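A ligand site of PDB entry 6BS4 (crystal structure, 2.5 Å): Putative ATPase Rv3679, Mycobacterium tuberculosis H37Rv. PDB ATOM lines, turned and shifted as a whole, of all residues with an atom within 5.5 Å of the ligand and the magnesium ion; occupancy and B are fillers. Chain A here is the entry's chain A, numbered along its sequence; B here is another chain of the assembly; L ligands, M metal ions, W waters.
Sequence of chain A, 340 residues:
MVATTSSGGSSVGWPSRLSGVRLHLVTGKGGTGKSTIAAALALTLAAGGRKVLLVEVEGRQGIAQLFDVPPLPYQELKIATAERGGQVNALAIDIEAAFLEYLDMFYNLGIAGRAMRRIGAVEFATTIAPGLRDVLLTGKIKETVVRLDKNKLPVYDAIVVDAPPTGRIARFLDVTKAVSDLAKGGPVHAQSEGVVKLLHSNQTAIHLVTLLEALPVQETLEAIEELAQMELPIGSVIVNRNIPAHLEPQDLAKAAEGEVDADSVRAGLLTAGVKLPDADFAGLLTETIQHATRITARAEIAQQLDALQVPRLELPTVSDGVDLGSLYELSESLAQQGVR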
ATOM      1  N   GLY A  28      32.469  14.632 -34.724  1.00  0.00           N
ATOM      2  CA  GLY A  28      33.056  15.947 -34.570  1.00  0.00           C
ATOM      3  C   GLY A  28      34.275  15.844 -33.671  1.00  0.00           C
ATOM      4  O   GLY A  28      34.409  14.869 -32.925  1.00  0.00           O
ATOM      5  N   LYS A  29      35.163  16.824 -33.743  1.00  0.00           N
ATOM      6  CA  LYS A  29      36.375  16.854 -32.940  1.00  0.00           C
ATOM      7  C   LYS A  29      36.044  16.796 -31.418  1.00  0.00           C
ATOM      8  O   LYS A  29      34.909  17.082 -31.027  1.00  0.00           O
ATOM      9  CB  LYS A  29      37.230  18.089 -33.302  1.00  0.00           C
ATOM     10  CG  LYS A  29      38.626  18.064 -32.712  1.00  0.00           C
ATOM     11  CD  LYS A  29      39.551  19.093 -33.344  1.00  0.00           C
ATOM     12  CE  LYS A  29      40.639  19.468 -32.375  1.00  0.00           C
ATOM     13  NZ  LYS A  29      41.550  18.334 -32.147  1.00  0.00           N
ATOM     14  N   GLY A  30      37.018  16.359 -30.604  1.00  0.00           N
ATOM     15  CA  GLY A  30      36.868  16.317 -29.162  1.00  0.00           C
ATOM     16  C   GLY A  30      36.470  17.678 -28.615  1.00  0.00           C
ATOM     17  O   GLY A  30      37.017  18.693 -29.038  1.00  0.00           O
ATOM     18  N   GLY A  31      35.489  17.698 -27.728  1.00  0.00           N
ATOM     19  CA  GLY A  31      34.992  18.912 -27.065  1.00  0.00           C
ATOM     20  C   GLY A  31      34.136  19.835 -27.906  1.00  0.00           C
ATOM     21  O   GLY A  31      33.884  20.964 -27.476  1.00  0.00           O
ATOM     22  N   THR A  32      33.682  19.394 -29.094  1.00  0.00           N
ATOM     23  CA  THR A  32      32.884  20.287 -29.969  1.00  0.00           C
ATOM     24  C   THR A  32      31.375  20.296 -29.660  1.00  0.00           C
ATOM     25  O   THR A  32      30.701  21.265 -29.986  1.00  0.00           O
ATOM     26  CB  THR A  32      33.141  20.029 -31.453  1.00  0.00           C
ATOM     27  OG1 THR A  32      32.863  18.664 -31.750  1.00  0.00           O
ATOM     28  CG2 THR A  32      34.552  20.407 -31.890  1.00  0.00           C
ATOM     29  N   GLY A  33      30.876  19.244 -29.018  1.00  0.00           N
ATOM     30  CA  GLY A  33      29.472  19.183 -28.617  1.00  0.00           C
ATOM     31  C   GLY A  33      28.726  17.911 -28.980  1.00  0.00           C
ATOM     32  O   GLY A  33      27.503  17.887 -28.837  1.00  0.00           O
ATOM     33  N   LYS A  34      29.436  16.845 -29.407  1.00  0.00           N
ATOM     34  CA  LYS A  34      28.833  15.558 -29.800  1.00  0.00           C
ATOM     35  C   LYS A  34      27.779  15.033 -28.834  1.00  0.00           C
ATOM     36  O   LYS A  34      26.643  14.779 -29.261  1.00  0.00           O
ATOM     37  CB  LYS A  34      29.901  14.463 -29.991  1.00  0.00           C
ATOM     38  CG  LYS A  34      30.799  14.606 -31.219  1.00  0.00           C
ATOM     39  CD  LYS A  34      31.795  13.424 -31.290  1.00  0.00           C
ATOM     40  CE  LYS A  34      32.839  13.414 -30.196  1.00  0.00           C
ATOM     41  NZ  LYS A  34      33.572  14.697 -30.089  1.00  0.00           N
ATOM     42  N   SER A  35      28.147  14.859 -27.555  1.00  0.00           N
ATOM     43  CA  SER A  35      27.252  14.319 -26.527  1.00  0.00           C
ATOM     44  C   SER A  35      26.013  15.180 -26.323  1.00  0.00           C
ATOM     45  O   SER A  35      24.897  14.666 -26.393  1.00  0.00           O
ATOM     46  CB  SER A  35      27.999  14.063 -25.217  1.00  0.00           C
ATOM     47  OG  SER A  35      29.067  13.142 -25.378  1.00  0.00           O
ATOM     48  N   THR A  36      26.207  16.485 -26.182  1.00  0.00           N
ATOM     49  CA  THR A  36      25.121  17.470 -25.996  1.00  0.00           C
ATOM     50  C   THR A  36      24.173  17.461 -27.171  1.00  0.00           C
ATOM     51  O   THR A  36      22.969  17.348 -26.971  1.00  0.00           O
ATOM     52  CB  THR A  36      25.740  18.867 -25.770  1.00  0.00           C
ATOM     53  OG1 THR A  36      26.662  18.790 -24.690  1.00  0.00           O
ATOM     54  CG2 THR A  36      24.705  19.918 -25.452  1.00  0.00           C
ATOM     55  N   ILE A  37      24.723  17.574 -28.398  1.00  0.00           N
ATOM     56  CA  ILE A  37      23.991  17.634 -29.658  1.00  0.00           C
ATOM     57  C   ILE A  37      23.265  16.309 -29.988  1.00  0.00           C
ATOM     58  O   ILE A  37      22.122  16.352 -30.430  1.00  0.00           O
ATOM     59  CB  ILE A  37      24.936  18.131 -30.770  1.00  0.00           C
ATOM     60  CG1 ILE A  37      25.365  19.592 -30.452  1.00  0.00           C
ATOM     61  CG2 ILE A  37      24.304  17.973 -32.176  1.00  0.00           C
ATOM     62  CD1 ILE A  37      26.095  20.384 -31.501  1.00  0.00           C
ATOM     63  N   GLU A  58      31.978   4.357 -26.401  1.00  0.00           N
ATOM     64  CA  GLU A  58      33.371   4.381 -25.912  1.00  0.00           C
ATOM     65  C   GLU A  58      33.588   3.989 -24.440  1.00  0.00           C
ATOM     66  O   GLU A  58      34.736   3.956 -23.990  1.00  0.00           O
ATOM     67  CB  GLU A  58      33.991   5.766 -26.207  1.00  0.00           C
ATOM     68  CG  GLU A  58      34.025   6.161 -27.684  1.00  0.00           C
ATOM     69  CD  GLU A  58      34.657   7.514 -27.956  1.00  0.00           C
ATOM     70  OE1 GLU A  58      34.187   8.521 -27.398  1.00  0.00           O
ATOM     71  OE2 GLU A  58      35.626   7.559 -28.760  1.00  0.00           O
ATOM     72  N   ARG A  60      32.734   5.670 -21.861  1.00  0.00           N
ATOM     73  CA  ARG A  60      33.020   6.905 -21.122  1.00  0.00           C
ATOM     74  C   ARG A  60      31.871   7.413 -20.281  1.00  0.00           C
ATOM     75  O   ARG A  60      32.062   8.371 -19.517  1.00  0.00           O
ATOM     76  CB  ARG A  60      33.519   7.983 -22.085  1.00  0.00           C
ATOM     77  CG  ARG A  60      34.882   7.638 -22.710  1.00  0.00           C
ATOM     78  CD  ARG A  60      35.211   8.596 -23.824  1.00  0.00           C
ATOM     79  NE  ARG A  60      35.207   9.968 -23.329  1.00  0.00           N
ATOM     80  CZ  ARG A  60      34.881  11.039 -24.050  1.00  0.00           C
ATOM     81  NH1 ARG A  60      34.531  10.900 -25.325  1.00  0.00           N
ATOM     82  NH2 ARG A  60      34.914  12.243 -23.504  1.00  0.00           N
ATOM     83  N   GLY A  62      29.246   9.157 -20.995  1.00  0.00           N
ATOM     84  CA  GLY A  62      28.931  10.535 -21.342  1.00  0.00           C
ATOM     85  C   GLY A  62      27.463  10.899 -21.227  1.00  0.00           C
ATOM     86  O   GLY A  62      27.155  12.070 -21.006  1.00  0.00           O
ATOM     87  N   GLN A  65      26.851  11.381 -17.422  1.00  0.00           N
ATOM     88  CA  GLN A  65      27.463  12.664 -17.103  1.00  0.00           C
ATOM     89  C   GLN A  65      26.596  13.838 -17.598  1.00  0.00           C
ATOM     90  O   GLN A  65      26.352  14.775 -16.857  1.00  0.00           O
ATOM     91  CB  GLN A  65      28.867  12.717 -17.692  1.00  0.00           C
ATOM     92  CG  GLN A  65      29.625  13.979 -17.310  1.00  0.00           C
ATOM     93  CD  GLN A  65      31.000  14.025 -17.911  1.00  0.00           C
ATOM     94  OE1 GLN A  65      31.991  13.676 -17.260  1.00  0.00           O
ATOM     95  NE2 GLN A  65      31.078  14.467 -19.164  1.00  0.00           N
ATOM     96  N   ASP A 162      25.963   8.931 -30.238  1.00  0.00           N
ATOM     97  CA  ASP A 162      26.964   9.886 -29.745  1.00  0.00           C
ATOM     98  C   ASP A 162      28.241   9.066 -30.114  1.00  0.00           C
ATOM     99  O   ASP A 162      28.609   8.110 -29.434  1.00  0.00           O
ATOM    100  CB  ASP A 162      26.807  10.050 -28.223  1.00  0.00           C
ATOM    101  CG  ASP A 162      27.874  10.837 -27.510  1.00  0.00           C
ATOM    102  OD1 ASP A 162      28.755  11.384 -28.189  1.00  0.00           O
ATOM    103  OD2 ASP A 162      27.823  10.915 -26.275  1.00  0.00           O
ATOM    104  N   PRO A 165      35.158  10.480 -32.200  1.00  0.00           N
ATOM    105  CA  PRO A 165      35.421  11.780 -32.855  1.00  0.00           C
ATOM    106  C   PRO A 165      35.845  11.700 -34.337  1.00  0.00           C
ATOM    107  O   PRO A 165      36.031  10.611 -34.867  1.00  0.00           O
ATOM    108  CB  PRO A 165      36.496  12.431 -31.967  1.00  0.00           C
ATOM    109  CG  PRO A 165      37.192  11.302 -31.306  1.00  0.00           C
ATOM    110  CD  PRO A 165      36.193  10.173 -31.182  1.00  0.00           C
ATOM    111  N   ASN A 240      28.124  24.462 -33.782  1.00  0.00           N
ATOM    112  CA  ASN A 240      27.773  24.686 -32.384  1.00  0.00           C
ATOM    113  C   ASN A 240      28.381  25.993 -31.860  1.00  0.00           C
ATOM    114  O   ASN A 240      29.333  26.533 -32.434  1.00  0.00           O
ATOM    115  CB  ASN A 240      28.246  23.490 -31.550  1.00  0.00           C
ATOM    116  CG  ASN A 240      27.668  23.371 -30.161  1.00  0.00           C
ATOM    117  OD1 ASN A 240      26.530  23.773 -29.884  1.00  0.00           O
ATOM    118  ND2 ASN A 240      28.443  22.794 -29.253  1.00  0.00           N
ATOM    119  N   ARG A 241      27.782  26.491 -30.750  1.00  0.00           N
ATOM    120  CA  ARG A 241      28.172  27.651 -29.949  1.00  0.00           C
ATOM    121  C   ARG A 241      28.413  28.901 -30.773  1.00  0.00           C
ATOM    122  O   ARG A 241      29.473  29.540 -30.722  1.00  0.00           O
ATOM    123  CB  ARG A 241      29.371  27.338 -29.034  1.00  0.00           C
ATOM    124  CG  ARG A 241      29.174  26.083 -28.231  1.00  0.00           C
ATOM    125  CD  ARG A 241      30.017  25.996 -26.990  1.00  0.00           C
ATOM    126  NE  ARG A 241      31.422  26.285 -27.244  1.00  0.00           N
ATOM    127  CZ  ARG A 241      32.369  26.224 -26.323  1.00  0.00           C
ATOM    128  NH1 ARG A 241      32.082  25.849 -25.082  1.00  0.00           N
ATOM    129  NH2 ARG A 241      33.620  26.530 -26.633  1.00  0.00           N
ATOM    130  N   LEU A 315      23.601  26.091 -33.978  1.00  0.00           N
ATOM    131  CA  LEU A 315      23.151  26.086 -32.591  1.00  0.00           C
ATOM    132  C   LEU A 315      23.763  27.266 -31.825  1.00  0.00           C
ATOM    133  O   LEU A 315      24.917  27.638 -32.076  1.00  0.00           O
ATOM    134  CB  LEU A 315      23.433  24.743 -31.909  1.00  0.00           C
ATOM    135  CG  LEU A 315      22.624  23.548 -32.448  1.00  0.00           C
ATOM    136  CD1 LEU A 315      23.059  22.277 -31.792  1.00  0.00           C
ATOM    137  CD2 LEU A 315      21.097  23.748 -32.232  1.00  0.00           C
ATOM    138  N   PRO A 316      22.990  27.920 -30.929  1.00  0.00           N
ATOM    139  CA  PRO A 316      23.557  29.047 -30.179  1.00  0.00           C
ATOM    140  C   PRO A 316      24.420  28.574 -29.002  1.00  0.00           C
ATOM    141  O   PRO A 316      24.509  27.367 -28.743  1.00  0.00           O
ATOM    142  CB  PRO A 316      22.304  29.770 -29.646  1.00  0.00           C
ATOM    143  CG  PRO A 316      21.327  28.648 -29.409  1.00  0.00           C
ATOM    144  CD  PRO A 316      21.593  27.649 -30.530  1.00  0.00           C
ATOM    145  N   THR A 317      25.032  29.530 -28.289  1.00  0.00           N
ATOM    146  CA  THR A 317      25.784  29.252 -27.077  1.00  0.00           C
ATOM    147  C   THR A 317      24.810  29.329 -25.909  1.00  0.00           C
ATOM    148  O   THR A 317      24.058  30.300 -25.793  1.00  0.00           O
ATOM    149  CB  THR A 317      26.903  30.293 -26.869  1.00  0.00           C
ATOM    150  OG1 THR A 317      27.753  30.309 -28.000  1.00  0.00           O
ATOM    151  CG2 THR A 317      27.721  30.034 -25.598  1.00  0.00           C
ATOM    152  N   VAL A 318      24.848  28.322 -25.025  1.00  0.00           N
ATOM    153  CA  VAL A 318      24.067  28.329 -23.792  1.00  0.00           C
ATOM    154  C   VAL A 318      24.924  29.158 -22.786  1.00  0.00           C
ATOM    155  O   VAL A 318      26.090  28.826 -22.524  1.00  0.00           O
ATOM    156  CB  VAL A 318      23.697  26.926 -23.275  1.00  0.00           C
ATOM    157  CG1 VAL A 318      23.078  27.007 -21.888  1.00  0.00           C
ATOM    158  CG2 VAL A 318      22.756  26.204 -24.248  1.00  0.00           C
ATOM    159  N   ASP A 320      24.922  29.683 -19.253  1.00  0.00           N
ATOM    160  CA  ASP A 320      25.471  28.944 -18.120  1.00  0.00           C
ATOM    161  C   ASP A 320      25.718  27.480 -18.467  1.00  0.00           C
ATOM    162  O   ASP A 320      25.567  27.082 -19.619  1.00  0.00           O
ATOM    163  CB  ASP A 320      24.542  29.058 -16.903  1.00  0.00           C
ATOM    164  CG  ASP A 320      24.454  30.473 -16.376  1.00  0.00           C
ATOM    165  OD1 ASP A 320      23.326  30.988 -16.243  1.00  0.00           O
ATOM    166  OD2 ASP A 320      25.514  31.067 -16.079  1.00  0.00           O
ATOM    167  N   VAL A 322      25.512  23.768 -19.383  1.00  0.00           N
ATOM    168  CA  VAL A 322      24.510  22.997 -20.131  1.00  0.00           C
ATOM    169  C   VAL A 322      23.832  22.107 -19.096  1.00  0.00           C
ATOM    170  O   VAL A 322      24.497  21.309 -18.441  1.00  0.00           O
ATOM    171  CB  VAL A 322      25.098  22.183 -21.327  1.00  0.00           C
ATOM    172  CG1 VAL A 322      24.117  21.118 -21.824  1.00  0.00           C
ATOM    173  CG2 VAL A 322      25.519  23.099 -22.468  1.00  0.00           C
ATOM    174  N   LEU A 330      18.202  23.599 -27.106  1.00  0.00           N
ATOM    175  CA  LEU A 330      18.954  23.182 -28.291  1.00  0.00           C
ATOM    176  C   LEU A 330      18.116  22.321 -29.204  1.00  0.00           C
ATOM    177  O   LEU A 330      18.215  22.475 -30.414  1.00  0.00           O
ATOM    178  CB  LEU A 330      20.287  22.498 -27.914  1.00  0.00           C
ATOM    179  CG  LEU A 330      21.269  23.326 -27.105  1.00  0.00           C
ATOM    180  CD1 LEU A 330      22.355  22.462 -26.553  1.00  0.00           C
ATOM    181  CD2 LEU A 330      21.842  24.517 -27.925  1.00  0.00           C
ATOM    182  N   ARG B 159      40.550  15.395 -21.806  1.00  0.00           N
ATOM    183  CA  ARG B 159      39.400  15.906 -21.044  1.00  0.00           C
ATOM    184  C   ARG B 159      39.796  15.799 -19.557  1.00  0.00           C
ATOM    185  O   ARG B 159      39.356  16.622 -18.747  1.00  0.00           O
ATOM    186  CB  ARG B 159      38.131  15.050 -21.356  1.00  0.00           C
ATOM    187  CG  ARG B 159      36.874  15.476 -20.591  1.00  0.00           C
ATOM    188  CD  ARG B 159      35.602  14.712 -20.948  1.00  0.00           C
ATOM    189  NE  ARG B 159      35.707  13.268 -20.761  1.00  0.00           N
ATOM    190  CZ  ARG B 159      35.384  12.619 -19.647  1.00  0.00           C
ATOM    191  NH1 ARG B 159      34.973  13.287 -18.575  1.00  0.00           N
ATOM    192  NH2 ARG B 159      35.505  11.297 -19.582  1.00  0.00           N
ATOM    193  N   ASP B 258      34.629  23.519 -16.881  1.00  0.00           N
ATOM    194  CA  ASP B 258      35.220  22.181 -17.113  1.00  0.00           C
ATOM    195  C   ASP B 258      36.750  22.213 -16.966  1.00  0.00           C
ATOM    196  O   ASP B 258      37.343  21.304 -16.346  1.00  0.00           O
ATOM    197  CB  ASP B 258      34.895  21.707 -18.547  1.00  0.00           C
ATOM    198  CG  ASP B 258      33.587  20.967 -18.802  1.00  0.00           C
ATOM    199  OD1 ASP B 258      32.766  20.846 -17.863  1.00  0.00           O
ATOM    200  OD2 ASP B 258      33.393  20.491 -19.952  1.00  0.00           O
HETATM  201  P1  LIG L   1      34.250  14.811 -25.850  1.00  0.00           P
HETATM  202  S1  LIG L   1      35.448  15.314 -24.467  1.00  0.00           S
HETATM  203  O1  LIG L   1      34.949  14.530 -27.232  1.00  0.00           O
HETATM  204  O2  LIG L   1      33.312  13.568 -25.700  1.00  0.00           O
HETATM  205  P2  LIG L   1      31.972  16.293 -26.936  1.00  0.00           P
HETATM  206  O3  LIG L   1      32.207  16.488 -28.382  1.00  0.00           O
HETATM  207  O4  LIG L   1      31.027  15.155 -26.497  1.00  0.00           O
HETATM  208  O5  LIG L   1      33.330  16.078 -26.123  1.00  0.00           O
HETATM  209  P3  LIG L   1      30.370  17.965 -25.142  1.00  0.00           P
HETATM  210  O6  LIG L   1      28.956  17.727 -25.536  1.00  0.00           O
HETATM  211  O7  LIG L   1      30.803  17.158 -23.888  1.00  0.00           O
HETATM  212  O8  LIG L   1      31.409  17.640 -26.296  1.00  0.00           O
HETATM  213  O9  LIG L   1      30.694  19.519 -24.984  1.00  0.00           O
HETATM  214  C1  LIG L   1      31.937  20.083 -24.507  1.00  0.00           C
HETATM  215  C2  LIG L   1      31.625  21.150 -23.486  1.00  0.00           C
HETATM  216  O10 LIG L   1      30.922  22.239 -24.116  1.00  0.00           O
HETATM  217  C3  LIG L   1      30.751  20.705 -22.311  1.00  0.00           C
HETATM  218  O11 LIG L   1      31.126  21.375 -21.116  1.00  0.00           O
HETATM  219  C4  LIG L   1      29.346  21.133 -22.743  1.00  0.00           C
HETATM  220  O12 LIG L   1      28.435  21.289 -21.666  1.00  0.00           O
HETATM  221  C5  LIG L   1      29.647  22.422 -23.504  1.00  0.00           C
HETATM  222  N1  LIG L   1      28.686  22.769 -24.556  1.00  0.00           N
HETATM  223  C6  LIG L   1      28.253  21.978 -25.594  1.00  0.00           C
HETATM  224  N2  LIG L   1      27.395  22.565 -26.403  1.00  0.00           N
HETATM  225  C7  LIG L   1      27.250  23.833 -25.860  1.00  0.00           C
HETATM  226  C8  LIG L   1      26.467  24.946 -26.224  1.00  0.00           C
HETATM  227  N3  LIG L   1      25.657  24.980 -27.289  1.00  0.00           N
HETATM  228  N4  LIG L   1      26.530  26.053 -25.443  1.00  0.00           N
HETATM  229  C9  LIG L   1      27.334  26.038 -24.374  1.00  0.00           C
HETATM  230  N5  LIG L   1      28.122  25.050 -23.929  1.00  0.00           N
HETATM  231  C10 LIG L   1      28.036  23.969 -24.717  1.00  0.00           C
HETATM  232 MG    MG M   1      31.294  13.284 -25.383  1.00  0.00          MG
HETATM  233  O   HOH W   1      35.629  12.318 -28.456  1.00  0.00           O
HETATM  234  O   HOH W   2      30.921  14.380 -23.629  1.00  0.00           O
HETATM  235  O   HOH W   3      31.326  11.686 -24.177  1.00  0.00           O
HETATM  236  O   HOH W   4      31.184  12.004 -27.103  1.00  0.00           O
HETATM  237  O   HOH W   5      31.606  22.499 -26.926  1.00  0.00           O
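One residue has an atom within 4 Å of the magnesium ion: Ser 35.
The nearest printed residue that does not touch the magnesium ion is Arg 60 (4.02 Å).
The backbone NH of Ser 35 sits close to an oxygen (O4) of the ligand (3.1 Å).
N of Thr 36 lies within hydrogen-bond range of O6 of the ligand (3.1 Å).
O6 of the ligand is in hydrogen-bond range of OG1 of Thr 36.
The side-chain carboxylate of Asp 258 of chain B is in hydrogen-bond range of an oxygen (O11) of the ligand (2.7 Å).
The backbone NH of Lys 34 sits at hydrogen-bond distance from an oxygen (O3) of the ligand.
An oxygen (O3) of the ligand lies within salt-bridge range of the side-chain amino group (NZ) of Lys 34 (2.8 Å).
The backbone NH of Val 318 is in hydrogen-bond range of a nitrogen (N4) of the ligand (2.9 Å).
The guanidinium group of Arg 60 sits close to a sulfur (S1) of the ligand (3.3 Å).
N3 of the ligand lies within hydrogen-bond range of OD1 of Asn 240.
The backbone carbonyl oxygen (O) of Pro 316 sits at hydrogen-bond distance from a nitrogen (N3) of the ligand, 3.0 Å away.
An oxygen (O3) of the ligand is in hydrogen-bond range of the backbone NH (N) of Gly 33 (3.1 Å).
N of Gly 31 is in hydrogen-bond range of O5 of the ligand (3.1 Å).
An oxygen (O3) of the ligand lies within hydrogen-bond range of the backbone NH (N) of Thr 32 (3.3 Å).
The side-chain hydroxyl (OG) of Ser 35 lies close to the side-chain carboxylate (OD2) of Asp 162, 2.7 Å away.
The side-chain amino group (NZ) of Lys 34 is in hydrogen-bond range of the backbone carbonyl oxygen (O) of Lys 29, at 2.9 Å.
NZ of Lys 34 sits at hydrogen-bond distance from O of Gly 28 (3.0 Å).
NH1 of Arg 60 is in salt-bridge range of OE1 of Glu 58, 3.2 Å away.
The side-chain amide nitrogen (ND2) of Asn 240 lies within hydrogen-bond range of the backbone carbonyl oxygen (O) of Thr 32 (2.8 Å).
O of Lys 29 lies within hydrogen-bond range of OG1 of Thr 32.
The side-chain hydroxyl of Thr 317 lies close to the backbone carbonyl oxygen of Arg 241 (3.3 Å).
NH1 of Arg 159 of chain B is in hydrogen-bond range of OE1 of Gln 65 (3.3 Å).
Lys 29 touches the ligand.
Gly 30 touches the ligand (CA to O1, 3.3 Å).
Arg 241 touches the ligand (CG to C8, 3.6 Å).
Thr 317 touches the ligand.
Val 322 touches the ligand (CB to O12, 3.5 Å).
CD2 of Leu 330 touches N3 of the ligand, at 3.9 Å.
Arg 159 of chain B touches the ligand.
Hydrophobic or aromatic side chains that line the ligand: Val 318, Val 322 and Leu 330.
Of the 27 residues printed, 18 come within 4 Å of the ligand.
The magnesium ion is bound by water W3, O2 of the ligand, water W2, water W4, O4 of the ligand and OG of Ser 35.
The magnesium ion has six donor atoms within binding distance.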
